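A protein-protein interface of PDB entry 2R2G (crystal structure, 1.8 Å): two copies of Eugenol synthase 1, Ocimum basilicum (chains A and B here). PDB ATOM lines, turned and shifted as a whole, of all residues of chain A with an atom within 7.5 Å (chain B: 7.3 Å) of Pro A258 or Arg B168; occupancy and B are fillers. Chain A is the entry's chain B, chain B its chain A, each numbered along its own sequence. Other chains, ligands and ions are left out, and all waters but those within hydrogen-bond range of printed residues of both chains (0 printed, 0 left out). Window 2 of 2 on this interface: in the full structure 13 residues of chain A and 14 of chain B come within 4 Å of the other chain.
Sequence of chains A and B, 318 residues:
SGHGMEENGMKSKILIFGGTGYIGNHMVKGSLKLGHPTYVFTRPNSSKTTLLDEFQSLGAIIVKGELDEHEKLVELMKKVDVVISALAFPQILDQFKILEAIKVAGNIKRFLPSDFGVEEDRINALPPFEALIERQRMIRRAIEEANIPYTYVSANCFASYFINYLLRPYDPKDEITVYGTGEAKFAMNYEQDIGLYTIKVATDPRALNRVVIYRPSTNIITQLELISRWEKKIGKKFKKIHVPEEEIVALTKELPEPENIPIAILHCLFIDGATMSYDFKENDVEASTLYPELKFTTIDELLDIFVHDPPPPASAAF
O of Tyr B165 is in hydrogen-bond range of NE of Arg B168 (2.7 Å). N of Lys B173 sits at hydrogen-bond distance from OD1 of Asp B171 (2.9 Å). The backbone carbonyl oxygen of Leu A255 sits at hydrogen-bond distance from the side-chain amide nitrogen of Asn A260 (3.5 Å).
Of the printed residues of chain B, Glu A259 touches Arg B168. Arg B168 touches just these residues of chain A: Glu A257 (3.1 Å), Pro A258 (3.5 Å) and Glu A259 (2.7 Å). Of the printed residues of chain A, Lys B173 touches Pro A256 (3.3 Å). Printed residues of chain A within 4 Å of Thr B177: Leu A255 (3.9 Å) and Pro A256 (3.2 Å). The nearest residue of chain B that does not touch Pro A258 is Tyr B170 (5.5 Å). The nearest printed residue of chain B that does not touch Glu A257 is Asp B171 (4.3 Å).
The backbone carbonyl oxygen (O) of Glu A257 lies within hydrogen-bond range of the guanidinium group (NH1) of Arg B168 (3.1 Å). The guanidinium group (NH2) of Arg B168 is in salt-bridge range of the side-chain carboxylate (OE2) of Glu A259 (2.7 Å). The backbone nitrogen (N) of Pro A256 sits close to the side-chain hydroxyl (OG1) of Thr B177, 3.4 Å away.
Of the 20 printed residues of chain B, 4 touch a printed residue of chain A. Printed residues of chain B that touch a printed residue of chain A: Arg B168, Lys B173, Thr B177 and Tyr B179. Hydrophobic or aromatic side chains of chain B that line the printed part of chain A: Tyr B179. Along chain B the printed residues that touch a printed residue of chain A span positions 168 to 179. Hydrophobic or aromatic side chains of chain A that line the printed part of chain B: Pro A256 and Pro A258. Along chain A the printed residues that touch a printed residue of chain B span positions 255 to 259.
No position is printed for both chains. Of the 7 pairs that touch across the chains among the printed residues, none has its exchanged pair printed and touching as well.
Among the printed residues, pairs that only touch across the chains: Pro A256 with Lys B173 (3.3 Å), Pro A258 with Arg B168 (3.5 Å), Leu A255 with Thr B177 (3.9 Å) and Pro A256 with Tyr B179 (3.9 Å).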
ATOM      1  N   PRO A 128      12.413  22.926   4.465  1.00  0.00           N
ATOM      2  CA  PRO A 128      13.444  23.533   3.616  1.00  0.00           C
ATOM      3  C   PRO A 128      13.702  25.009   3.919  1.00  0.00           C
ATOM      4  O   PRO A 128      14.848  25.460   3.912  1.00  0.00           O
ATOM      5  CB  PRO A 128      12.903  23.311   2.206  1.00  0.00           C
ATOM      6  CG  PRO A 128      12.166  22.006   2.343  1.00  0.00           C
ATOM      7  CD  PRO A 128      11.418  22.207   3.649  1.00  0.00           C
ATOM      8  N   LEU A 255      12.312  16.541  -3.711  1.00  0.00           N
ATOM      9  CA  LEU A 255      13.374  17.198  -4.443  1.00  0.00           C
ATOM     10  C   LEU A 255      14.528  17.475  -3.504  1.00  0.00           C
ATOM     11  O   LEU A 255      14.325  17.820  -2.345  1.00  0.00           O
ATOM     12  CB  LEU A 255      12.889  18.506  -5.071  1.00  0.00           C
ATOM     13  CG  LEU A 255      11.826  18.405  -6.170  1.00  0.00           C
ATOM     14  CD1 LEU A 255      11.507  19.775  -6.748  1.00  0.00           C
ATOM     15  CD2 LEU A 255      12.365  17.491  -7.267  1.00  0.00           C
ATOM     16  N   PRO A 256      15.775  17.326  -3.983  1.00  0.00           N
ATOM     17  CA  PRO A 256      16.962  17.574  -3.138  1.00  0.00           C
ATOM     18  C   PRO A 256      17.195  19.066  -2.943  1.00  0.00           C
ATOM     19  O   PRO A 256      16.541  19.891  -3.572  1.00  0.00           O
ATOM     20  CB  PRO A 256      18.099  16.963  -3.966  1.00  0.00           C
ATOM     21  CG  PRO A 256      17.643  17.266  -5.369  1.00  0.00           C
ATOM     22  CD  PRO A 256      16.184  16.875  -5.332  1.00  0.00           C
ATOM     23  N   GLU A 257      18.143  19.393  -2.062  1.00  0.00           N
ATOM     24  CA  GLU A 257      18.512  20.797  -1.819  1.00  0.00           C
ATOM     25  C   GLU A 257      19.544  21.136  -2.912  1.00  0.00           C
ATOM     26  O   GLU A 257      20.292  20.273  -3.355  1.00  0.00           O
ATOM     27  CB  GLU A 257      19.158  20.950  -0.450  1.00  0.00           C
ATOM     28  CG  GLU A 257      18.183  20.738   0.724  1.00  0.00           C
ATOM     29  CD  GLU A 257      18.874  20.852   2.063  1.00  0.00           C
ATOM     30  OE1 GLU A 257      19.778  20.029   2.340  1.00  0.00           O
ATOM     31  OE2 GLU A 257      18.523  21.787   2.817  1.00  0.00           O
ATOM     32  N   PRO A 258      19.594  22.402  -3.356  1.00  0.00           N
ATOM     33  CA  PRO A 258      18.813  23.590  -2.997  1.00  0.00           C
ATOM     34  C   PRO A 258      17.450  23.715  -3.673  1.00  0.00           C
ATOM     35  O   PRO A 258      16.634  24.560  -3.295  1.00  0.00           O
ATOM     36  CB  PRO A 258      19.737  24.738  -3.369  1.00  0.00           C
ATOM     37  CG  PRO A 258      20.419  24.211  -4.598  1.00  0.00           C
ATOM     38  CD  PRO A 258      20.670  22.750  -4.284  1.00  0.00           C
ATOM     39  N   GLU A 259      17.223  22.894  -4.693  1.00  0.00           N
ATOM     40  CA  GLU A 259      15.983  22.904  -5.455  1.00  0.00           C
ATOM     41  C   GLU A 259      14.694  23.031  -4.637  1.00  0.00           C
ATOM     42  O   GLU A 259      13.790  23.775  -5.008  1.00  0.00           O
ATOM     43  CB  GLU A 259      15.890  21.647  -6.333  1.00  0.00           C
ATOM     44  CG  GLU A 259      16.883  21.571  -7.491  1.00  0.00           C
ATOM     45  CD  GLU A 259      18.305  21.245  -7.058  1.00  0.00           C
ATOM     46  OE1 GLU A 259      18.533  21.006  -5.854  1.00  0.00           O
ATOM     47  OE2 GLU A 259      19.200  21.225  -7.935  1.00  0.00           O
ATOM     48  N   ASN A 260      14.596  22.316  -3.520  1.00  0.00           N
ATOM     49  CA  ASN A 260      13.379  22.359  -2.715  1.00  0.00           C
ATOM     50  C   ASN A 260      13.172  23.626  -1.884  1.00  0.00           C
ATOM     51  O   ASN A 260      12.082  23.846  -1.362  1.00  0.00           O
ATOM     52  CB  ASN A 260      13.296  21.127  -1.801  1.00  0.00           C
ATOM     53  CG  ASN A 260      14.315  21.151  -0.689  1.00  0.00           C
ATOM     54  OD1 ASN A 260      15.182  22.020  -0.644  1.00  0.00           O
ATOM     55  ND2 ASN A 260      14.224  20.185   0.219  1.00  0.00           N
ATOM     56  N   ILE A 261      14.198  24.463  -1.763  1.00  0.00           N
ATOM     57  CA  ILE A 261      14.064  25.692  -0.979  1.00  0.00           C
ATOM     58  C   ILE A 261      13.106  26.720  -1.620  1.00  0.00           C
ATOM     59  O   ILE A 261      12.200  27.236  -0.960  1.00  0.00           O
ATOM     60  CB  ILE A 261      15.443  26.350  -0.739  1.00  0.00           C
ATOM     61  CG1 ILE A 261      16.357  25.386   0.023  1.00  0.00           C
ATOM     62  CG2 ILE A 261      15.275  27.630   0.069  1.00  0.00           C
ATOM     63  CD1 ILE A 261      17.758  25.925   0.268  1.00  0.00           C
ATOM     64  N   PRO A 262      13.293  27.034  -2.914  1.00  0.00           N
ATOM     65  CA  PRO A 262      12.396  28.008  -3.554  1.00  0.00           C
ATOM     66  C   PRO A 262      10.940  27.540  -3.483  1.00  0.00           C
ATOM     67  O   PRO A 262      10.021  28.337  -3.277  1.00  0.00           O
ATOM     68  CB  PRO A 262      12.897  28.053  -4.997  1.00  0.00           C
ATOM     69  CG  PRO A 262      14.343  27.685  -4.874  1.00  0.00           C
ATOM     70  CD  PRO A 262      14.329  26.575  -3.857  1.00  0.00           C
ATOM     71  N   ILE A 263      10.747  26.236  -3.661  1.00  0.00           N
ATOM     72  CA  ILE A 263       9.414  25.647  -3.618  1.00  0.00           C
ATOM     73  C   ILE A 263       8.785  25.895  -2.247  1.00  0.00           C
ATOM     74  O   ILE A 263       7.630  26.312  -2.152  1.00  0.00           O
ATOM     75  CB  ILE A 263       9.477  24.121  -3.920  1.00  0.00           C
ATOM     76  CG1 ILE A 263       9.933  23.898  -5.364  1.00  0.00           C
ATOM     77  CG2 ILE A 263       8.116  23.474  -3.701  1.00  0.00           C
ATOM     78  CD1 ILE A 263       8.977  24.466  -6.405  1.00  0.00           C
ATOM     79  N   ALA A 264       9.549  25.652  -1.186  1.00  0.00           N
ATOM     80  CA  ALA A 264       9.044  25.862   0.170  1.00  0.00           C
ATOM     81  C   ALA A 264       8.704  27.335   0.414  1.00  0.00           C
ATOM     82  O   ALA A 264       7.730  27.659   1.105  1.00  0.00           O
ATOM     83  CB  ALA A 264      10.072  25.381   1.198  1.00  0.00           C
ATOM     84  N   ALA A 317      20.471  33.164  -4.401  1.00  0.00           N
ATOM     85  CA  ALA A 317      21.431  32.076  -4.245  1.00  0.00           C
ATOM     86  C   ALA A 317      20.993  31.138  -3.125  1.00  0.00           C
ATOM     87  O   ALA A 317      20.544  31.588  -2.070  1.00  0.00           O
ATOM     88  CB  ALA A 317      22.816  32.641  -3.940  1.00  0.00           C
ATOM     89  N   PHE A 318      21.122  29.835  -3.361  1.00  0.00           N
ATOM     90  CA  PHE A 318      20.745  28.838  -2.364  1.00  0.00           C
ATOM     91  C   PHE A 318      21.823  27.769  -2.222  1.00  0.00           C
ATOM     92  O   PHE A 318      22.772  27.805  -3.036  1.00  0.00           O
ATOM     93  CB  PHE A 318      19.414  28.183  -2.743  1.00  0.00           C
ATOM     94  CG  PHE A 318      18.279  29.153  -2.860  1.00  0.00           C
ATOM     95  CD1 PHE A 318      17.915  29.949  -1.778  1.00  0.00           C
ATOM     96  CD2 PHE A 318      17.584  29.293  -4.057  1.00  0.00           C
ATOM     97  CE1 PHE A 318      16.880  30.871  -1.885  1.00  0.00           C
ATOM     98  CE2 PHE A 318      16.545  30.213  -4.174  1.00  0.00           C
ATOM     99  CZ  PHE A 318      16.195  31.002  -3.086  1.00  0.00           C
ATOM    100  N   PHE B 162      26.548  15.398 -14.253  1.00  0.00           N
ATOM    101  CA  PHE B 162      25.523  14.559 -13.664  1.00  0.00           C
ATOM    102  C   PHE B 162      25.897  13.812 -12.409  1.00  0.00           C
ATOM    103  O   PHE B 162      25.019  13.452 -11.618  1.00  0.00           O
ATOM    104  CB  PHE B 162      24.915  13.647 -14.728  1.00  0.00           C
ATOM    105  CG  PHE B 162      23.934  14.373 -15.607  1.00  0.00           C
ATOM    106  CD1 PHE B 162      24.328  14.909 -16.832  1.00  0.00           C
ATOM    107  CD2 PHE B 162      22.643  14.619 -15.152  1.00  0.00           C
ATOM    108  CE1 PHE B 162      23.443  15.686 -17.583  1.00  0.00           C
ATOM    109  CE2 PHE B 162      21.747  15.395 -15.896  1.00  0.00           C
ATOM    110  CZ  PHE B 162      22.147  15.929 -17.109  1.00  0.00           C
ATOM    111  N   ILE B 163      27.187  13.588 -12.190  1.00  0.00           N
ATOM    112  CA  ILE B 163      27.576  12.944 -10.941  1.00  0.00           C
ATOM    113  C   ILE B 163      27.284  14.014  -9.873  1.00  0.00           C
ATOM    114  O   ILE B 163      26.729  13.717  -8.813  1.00  0.00           O
ATOM    115  CB  ILE B 163      29.070  12.524 -10.963  1.00  0.00           C
ATOM    116  CG1 ILE B 163      29.221  11.257 -11.818  1.00  0.00           C
ATOM    117  CG2 ILE B 163      29.572  12.268  -9.548  1.00  0.00           C
ATOM    118  CD1 ILE B 163      30.654  10.836 -12.092  1.00  0.00           C
ATOM    119  N   ASN B 164      27.617  15.269 -10.174  1.00  0.00           N
ATOM    120  CA  ASN B 164      27.348  16.360  -9.235  1.00  0.00           C
ATOM    121  C   ASN B 164      25.855  16.518  -9.003  1.00  0.00           C
ATOM    122  O   ASN B 164      25.407  16.659  -7.869  1.00  0.00           O
ATOM    123  CB  ASN B 164      27.906  17.695  -9.753  1.00  0.00           C
ATOM    124  CG  ASN B 164      29.340  17.935  -9.323  1.00  0.00           C
ATOM    125  OD1 ASN B 164      29.676  17.790  -8.152  1.00  0.00           O
ATOM    126  ND2 ASN B 164      30.190  18.314 -10.270  1.00  0.00           N
ATOM    127  N   TYR B 165      25.083  16.482 -10.083  1.00  0.00           N
ATOM    128  CA  TYR B 165      23.642  16.646 -10.000  1.00  0.00           C
ATOM    129  C   TYR B 165      22.902  15.509  -9.287  1.00  0.00           C
ATOM    130  O   TYR B 165      22.004  15.757  -8.466  1.00  0.00           O
ATOM    131  CB  TYR B 165      23.070  16.807 -11.409  1.00  0.00           C
ATOM    132  CG  TYR B 165      21.666  17.348 -11.436  1.00  0.00           C
ATOM    133  CD1 TYR B 165      21.425  18.717 -11.339  1.00  0.00           C
ATOM    134  CD2 TYR B 165      20.574  16.492 -11.543  1.00  0.00           C
ATOM    135  CE1 TYR B 165      20.130  19.222 -11.352  1.00  0.00           C
ATOM    136  CE2 TYR B 165      19.275  16.983 -11.552  1.00  0.00           C
ATOM    137  CZ  TYR B 165      19.058  18.350 -11.458  1.00  0.00           C
ATOM    138  OH  TYR B 165      17.771  18.842 -11.487  1.00  0.00           O
ATOM    139  N   LEU B 166      23.278  14.269  -9.599  1.00  0.00           N
ATOM    140  CA  LEU B 166      22.625  13.101  -9.014  1.00  0.00           C
ATOM    141  C   LEU B 166      23.114  12.708  -7.624  1.00  0.00           C
ATOM    142  O   LEU B 166      22.306  12.405  -6.748  1.00  0.00           O
ATOM    143  CB  LEU B 166      22.765  11.884  -9.945  1.00  0.00           C
ATOM    144  CG  LEU B 166      22.081  11.922 -11.322  1.00  0.00           C
ATOM    145  CD1 LEU B 166      22.462  10.676 -12.119  1.00  0.00           C
ATOM    146  CD2 LEU B 166      20.569  11.996 -11.157  1.00  0.00           C
ATOM    147  N   LEU B 167      24.427  12.707  -7.424  1.00  0.00           N
ATOM    148  CA  LEU B 167      24.995  12.306  -6.144  1.00  0.00           C
ATOM    149  C   LEU B 167      25.241  13.449  -5.170  1.00  0.00           C
ATOM    150  O   LEU B 167      25.425  13.206  -3.981  1.00  0.00           O
ATOM    151  CB  LEU B 167      26.311  11.541  -6.354  1.00  0.00           C
ATOM    152  CG  LEU B 167      26.264  10.284  -7.231  1.00  0.00           C
ATOM    153  CD1 LEU B 167      27.642   9.646  -7.272  1.00  0.00           C
ATOM    154  CD2 LEU B 167      25.233   9.298  -6.682  1.00  0.00           C
ATOM    155  N   ARG B 168      25.249  14.684  -5.668  1.00  0.00           N
ATOM    156  CA  ARG B 168      25.488  15.848  -4.815  1.00  0.00           C
ATOM    157  C   ARG B 168      26.597  15.508  -3.812  1.00  0.00           C
ATOM    158  O   ARG B 168      26.417  15.650  -2.602  1.00  0.00           O
ATOM    159  CB  ARG B 168      24.207  16.214  -4.058  1.00  0.00           C
ATOM    160  CG  ARG B 168      22.979  16.364  -4.943  1.00  0.00           C
ATOM    161  CD  ARG B 168      22.929  17.721  -5.628  1.00  0.00           C
ATOM    162  NE  ARG B 168      21.946  17.746  -6.707  1.00  0.00           N
ATOM    163  CZ  ARG B 168      21.178  18.791  -6.999  1.00  0.00           C
ATOM    164  NH1 ARG B 168      21.275  19.905  -6.283  1.00  0.00           N
ATOM    165  NH2 ARG B 168      20.318  18.723  -8.007  1.00  0.00           N
ATOM    166  N   PRO B 169      27.760  15.054  -4.310  1.00  0.00           N
ATOM    167  CA  PRO B 169      28.908  14.679  -3.475  1.00  0.00           C
ATOM    168  C   PRO B 169      29.389  15.750  -2.505  1.00  0.00           C
ATOM    169  O   PRO B 169      30.035  15.443  -1.507  1.00  0.00           O
ATOM    170  CB  PRO B 169      29.974  14.304  -4.504  1.00  0.00           C
ATOM    171  CG  PRO B 169      29.616  15.149  -5.685  1.00  0.00           C
ATOM    172  CD  PRO B 169      28.122  15.007  -5.737  1.00  0.00           C
ATOM    173  N   TYR B 170      29.074  17.003  -2.801  1.00  0.00           N
ATOM    174  CA  TYR B 170      29.472  18.115  -1.949  1.00  0.00           C
ATOM    175  C   TYR B 170      28.390  18.404  -0.915  1.00  0.00           C
ATOM    176  O   TYR B 170      28.378  19.468  -0.292  1.00  0.00           O
ATOM    177  CB  TYR B 170      29.727  19.355  -2.808  1.00  0.00           C
ATOM    178  CG  TYR B 170      28.571  19.699  -3.712  1.00  0.00           C
ATOM    179  CD1 TYR B 170      27.458  20.385  -3.225  1.00  0.00           C
ATOM    180  CD2 TYR B 170      28.562  19.293  -5.047  1.00  0.00           C
ATOM    181  CE1 TYR B 170      26.364  20.652  -4.044  1.00  0.00           C
ATOM    182  CE2 TYR B 170      27.475  19.554  -5.872  1.00  0.00           C
ATOM    183  CZ  TYR B 170      26.379  20.232  -5.363  1.00  0.00           C
ATOM    184  OH  TYR B 170      25.293  20.475  -6.171  1.00  0.00           O
ATOM    185  N   ASP B 171      27.478  17.450  -0.742  1.00  0.00           N
ATOM    186  CA  ASP B 171      26.383  17.584   0.216  1.00  0.00           C
ATOM    187  C   ASP B 171      26.436  16.430   1.217  1.00  0.00           C
ATOM    188  O   ASP B 171      26.347  15.261   0.842  1.00  0.00           O
ATOM    189  CB  ASP B 171      25.038  17.568  -0.518  1.00  0.00           C
ATOM    190  CG  ASP B 171      23.888  18.038   0.355  1.00  0.00           C
ATOM    191  OD1 ASP B 171      23.787  17.584   1.515  1.00  0.00           O
ATOM    192  OD2 ASP B 171      23.078  18.859  -0.127  1.00  0.00           O
ATOM    193  N   PRO B 172      26.573  16.744   2.510  1.00  0.00           N
ATOM    194  CA  PRO B 172      26.638  15.716   3.554  1.00  0.00           C
ATOM    195  C   PRO B 172      25.302  15.077   3.946  1.00  0.00           C
ATOM    196  O   PRO B 172      25.222  14.391   4.969  1.00  0.00           O
ATOM    197  CB  PRO B 172      27.277  16.464   4.719  1.00  0.00           C
ATOM    198  CG  PRO B 172      26.706  17.839   4.563  1.00  0.00           C
ATOM    199  CD  PRO B 172      26.836  18.081   3.073  1.00  0.00           C
ATOM    200  N   LYS B 173      24.263  15.288   3.141  1.00  0.00           N
ATOM    201  CA  LYS B 173      22.937  14.736   3.437  1.00  0.00           C
ATOM    202  C   LYS B 173      22.904  13.204   3.500  1.00  0.00           C
ATOM    203  O   LYS B 173      23.765  12.531   2.935  1.00  0.00           O
ATOM    204  CB  LYS B 173      21.923  15.227   2.400  1.00  0.00           C
ATOM    205  CG  LYS B 173      22.240  14.800   0.980  1.00  0.00           C
ATOM    206  CD  LYS B 173      21.225  15.347  -0.005  1.00  0.00           C
ATOM    207  CE  LYS B 173      21.541  14.908  -1.427  1.00  0.00           C
ATOM    208  NZ  LYS B 173      20.598  15.536  -2.395  1.00  0.00           N
ATOM    209  N   GLU B 175      20.089  11.446   2.558  1.00  0.00           N
ATOM    210  CA  GLU B 175      19.138  10.960   1.563  1.00  0.00           C
ATOM    211  C   GLU B 175      19.589  11.326   0.161  1.00  0.00           C
ATOM    212  O   GLU B 175      20.384  12.251  -0.028  1.00  0.00           O
ATOM    213  CB  GLU B 175      17.753  11.563   1.785  1.00  0.00           C
ATOM    214  CG  GLU B 175      17.192  11.375   3.173  1.00  0.00           C
ATOM    215  CD  GLU B 175      17.098  12.683   3.927  1.00  0.00           C
ATOM    216  OE1 GLU B 175      18.153  13.315   4.157  1.00  0.00           O
ATOM    217  OE2 GLU B 175      15.966  13.082   4.284  1.00  0.00           O
ATOM    218  N   ILE B 176      19.075  10.593  -0.818  1.00  0.00           N
ATOM    219  CA  ILE B 176      19.390  10.854  -2.213  1.00  0.00           C
ATOM    220  C   ILE B 176      18.114  10.740  -3.017  1.00  0.00           C
ATOM    221  O   ILE B 176      17.319   9.823  -2.811  1.00  0.00           O
ATOM    222  CB  ILE B 176      20.419   9.857  -2.784  1.00  0.00           C
ATOM    223  CG1 ILE B 176      21.801  10.142  -2.202  1.00  0.00           C
ATOM    224  CG2 ILE B 176      20.479   9.987  -4.306  1.00  0.00           C
ATOM    225  CD1 ILE B 176      22.920   9.395  -2.910  1.00  0.00           C
ATOM    226  N   THR B 177      17.925  11.686  -3.927  1.00  0.00           N
ATOM    227  CA  THR B 177      16.751  11.717  -4.781  1.00  0.00           C
ATOM    228  C   THR B 177      16.954  10.855  -6.031  1.00  0.00           C
ATOM    229  O   THR B 177      17.974  10.953  -6.702  1.00  0.00           O
ATOM    230  CB  THR B 177      16.435  13.164  -5.216  1.00  0.00           C
ATOM    231  OG1 THR B 177      16.067  13.938  -4.064  1.00  0.00           O
ATOM    232  CG2 THR B 177      15.303  13.186  -6.228  1.00  0.00           C
ATOM    233  N   TYR B 179      15.056   9.683  -9.654  1.00  0.00           N
ATOM    234  CA  TYR B 179      14.002  10.079 -10.579  1.00  0.00           C
ATOM    235  C   TYR B 179      13.391   8.842 -11.212  1.00  0.00           C
ATOM    236  O   TYR B 179      14.083   8.053 -11.858  1.00  0.00           O
ATOM    237  CB  TYR B 179      14.588  11.010 -11.635  1.00  0.00           C
ATOM    238  CG  TYR B 179      15.154  12.257 -11.010  1.00  0.00           C
ATOM    239  CD1 TYR B 179      14.310  13.257 -10.527  1.00  0.00           C
ATOM    240  CD2 TYR B 179      16.525  12.404 -10.821  1.00  0.00           C
ATOM    241  CE1 TYR B 179      14.817  14.374  -9.864  1.00  0.00           C
ATOM    242  CE2 TYR B 179      17.045  13.516 -10.155  1.00  0.00           C
ATOM    243  CZ  TYR B 179      16.183  14.495  -9.678  1.00  0.00           C
ATOM    244  OH  TYR B 179      16.685  15.583  -8.994  1.00  0.00           O
ATOM    245  N   TRP B 230      28.874   4.378  -5.579  1.00  0.00           N
ATOM    246  CA  TRP B 230      29.347   5.546  -4.837  1.00  0.00           C
ATOM    247  C   TRP B 230      29.336   5.207  -3.346  1.00  0.00           C
ATOM    248  O   TRP B 230      30.266   5.548  -2.603  1.00  0.00           O
ATOM    249  CB  TRP B 230      28.422   6.739  -5.091  1.00  0.00           C
ATOM    250  CG  TRP B 230      28.781   7.972  -4.314  1.00  0.00           C
ATOM    251  CD1 TRP B 230      27.960   8.666  -3.469  1.00  0.00           C
ATOM    252  CD2 TRP B 230      30.015   8.704  -4.366  1.00  0.00           C
ATOM    253  NE1 TRP B 230      28.602   9.781  -2.997  1.00  0.00           N
ATOM    254  CE2 TRP B 230      29.865   9.830  -3.526  1.00  0.00           C
ATOM    255  CE3 TRP B 230      31.234   8.516  -5.034  1.00  0.00           C
ATOM    256  CZ2 TRP B 230      30.884  10.776  -3.343  1.00  0.00           C
ATOM    257  CZ3 TRP B 230      32.253   9.459  -4.853  1.00  0.00           C
ATOM    258  CH2 TRP B 230      32.070  10.571  -4.009  1.00  0.00           C
ATOM    259  N   PHE B 238      22.851   5.690   1.759  1.00  0.00           N
ATOM    260  CA  PHE B 238      21.865   6.756   1.601  1.00  0.00           C
ATOM    261  C   PHE B 238      20.447   6.216   1.590  1.00  0.00           C
ATOM    262  O   PHE B 238      20.216   5.063   1.248  1.00  0.00           O
ATOM    263  CB  PHE B 238      22.090   7.505   0.279  1.00  0.00           C
ATOM    264  CG  PHE B 238      23.426   8.174   0.174  1.00  0.00           C
ATOM    265  CD1 PHE B 238      23.651   9.406   0.774  1.00  0.00           C
ATOM    266  CD2 PHE B 238      24.475   7.547  -0.488  1.00  0.00           C
ATOM    267  CE1 PHE B 238      24.907  10.008   0.722  1.00  0.00           C
ATOM    268  CE2 PHE B 238      25.734   8.135  -0.547  1.00  0.00           C
ATOM    269  CZ  PHE B 238      25.951   9.371   0.061  1.00  0.00           C
ATOM    270  N   LEU B 266      15.132  15.560 -17.386  1.00  0.00           N
ATOM    271  CA  LEU B 266      15.344  14.536 -16.374  1.00  0.00           C
ATOM    272  C   LEU B 266      14.484  13.325 -16.709  1.00  0.00           C
ATOM    273  O   LEU B 266      14.891  12.180 -16.513  1.00  0.00           O
ATOM    274  CB  LEU B 266      14.979  15.071 -14.988  1.00  0.00           C
ATOM    275  CG  LEU B 266      16.091  15.870 -14.305  1.00  0.00           C
ATOM    276  CD1 LEU B 266      15.577  16.467 -13.004  1.00  0.00           C
ATOM    277  CD2 LEU B 266      17.292  14.958 -14.049  1.00  0.00           C
ATOM    278  N   PRO B 313      30.157  21.756  -9.202  1.00  0.00           N
ATOM    279  CA  PRO B 313      28.902  21.511  -9.914  1.00  0.00           C
ATOM    280  C   PRO B 313      28.595  22.651 -10.881  1.00  0.00           C
ATOM    281  O   PRO B 313      29.113  23.759 -10.729  1.00  0.00           O
ATOM    282  CB  PRO B 313      27.882  21.417  -8.785  1.00  0.00           C
ATOM    283  CG  PRO B 313      28.432  22.382  -7.772  1.00  0.00           C
ATOM    284  CD  PRO B 313      29.905  22.047  -7.778  1.00  0.00           C
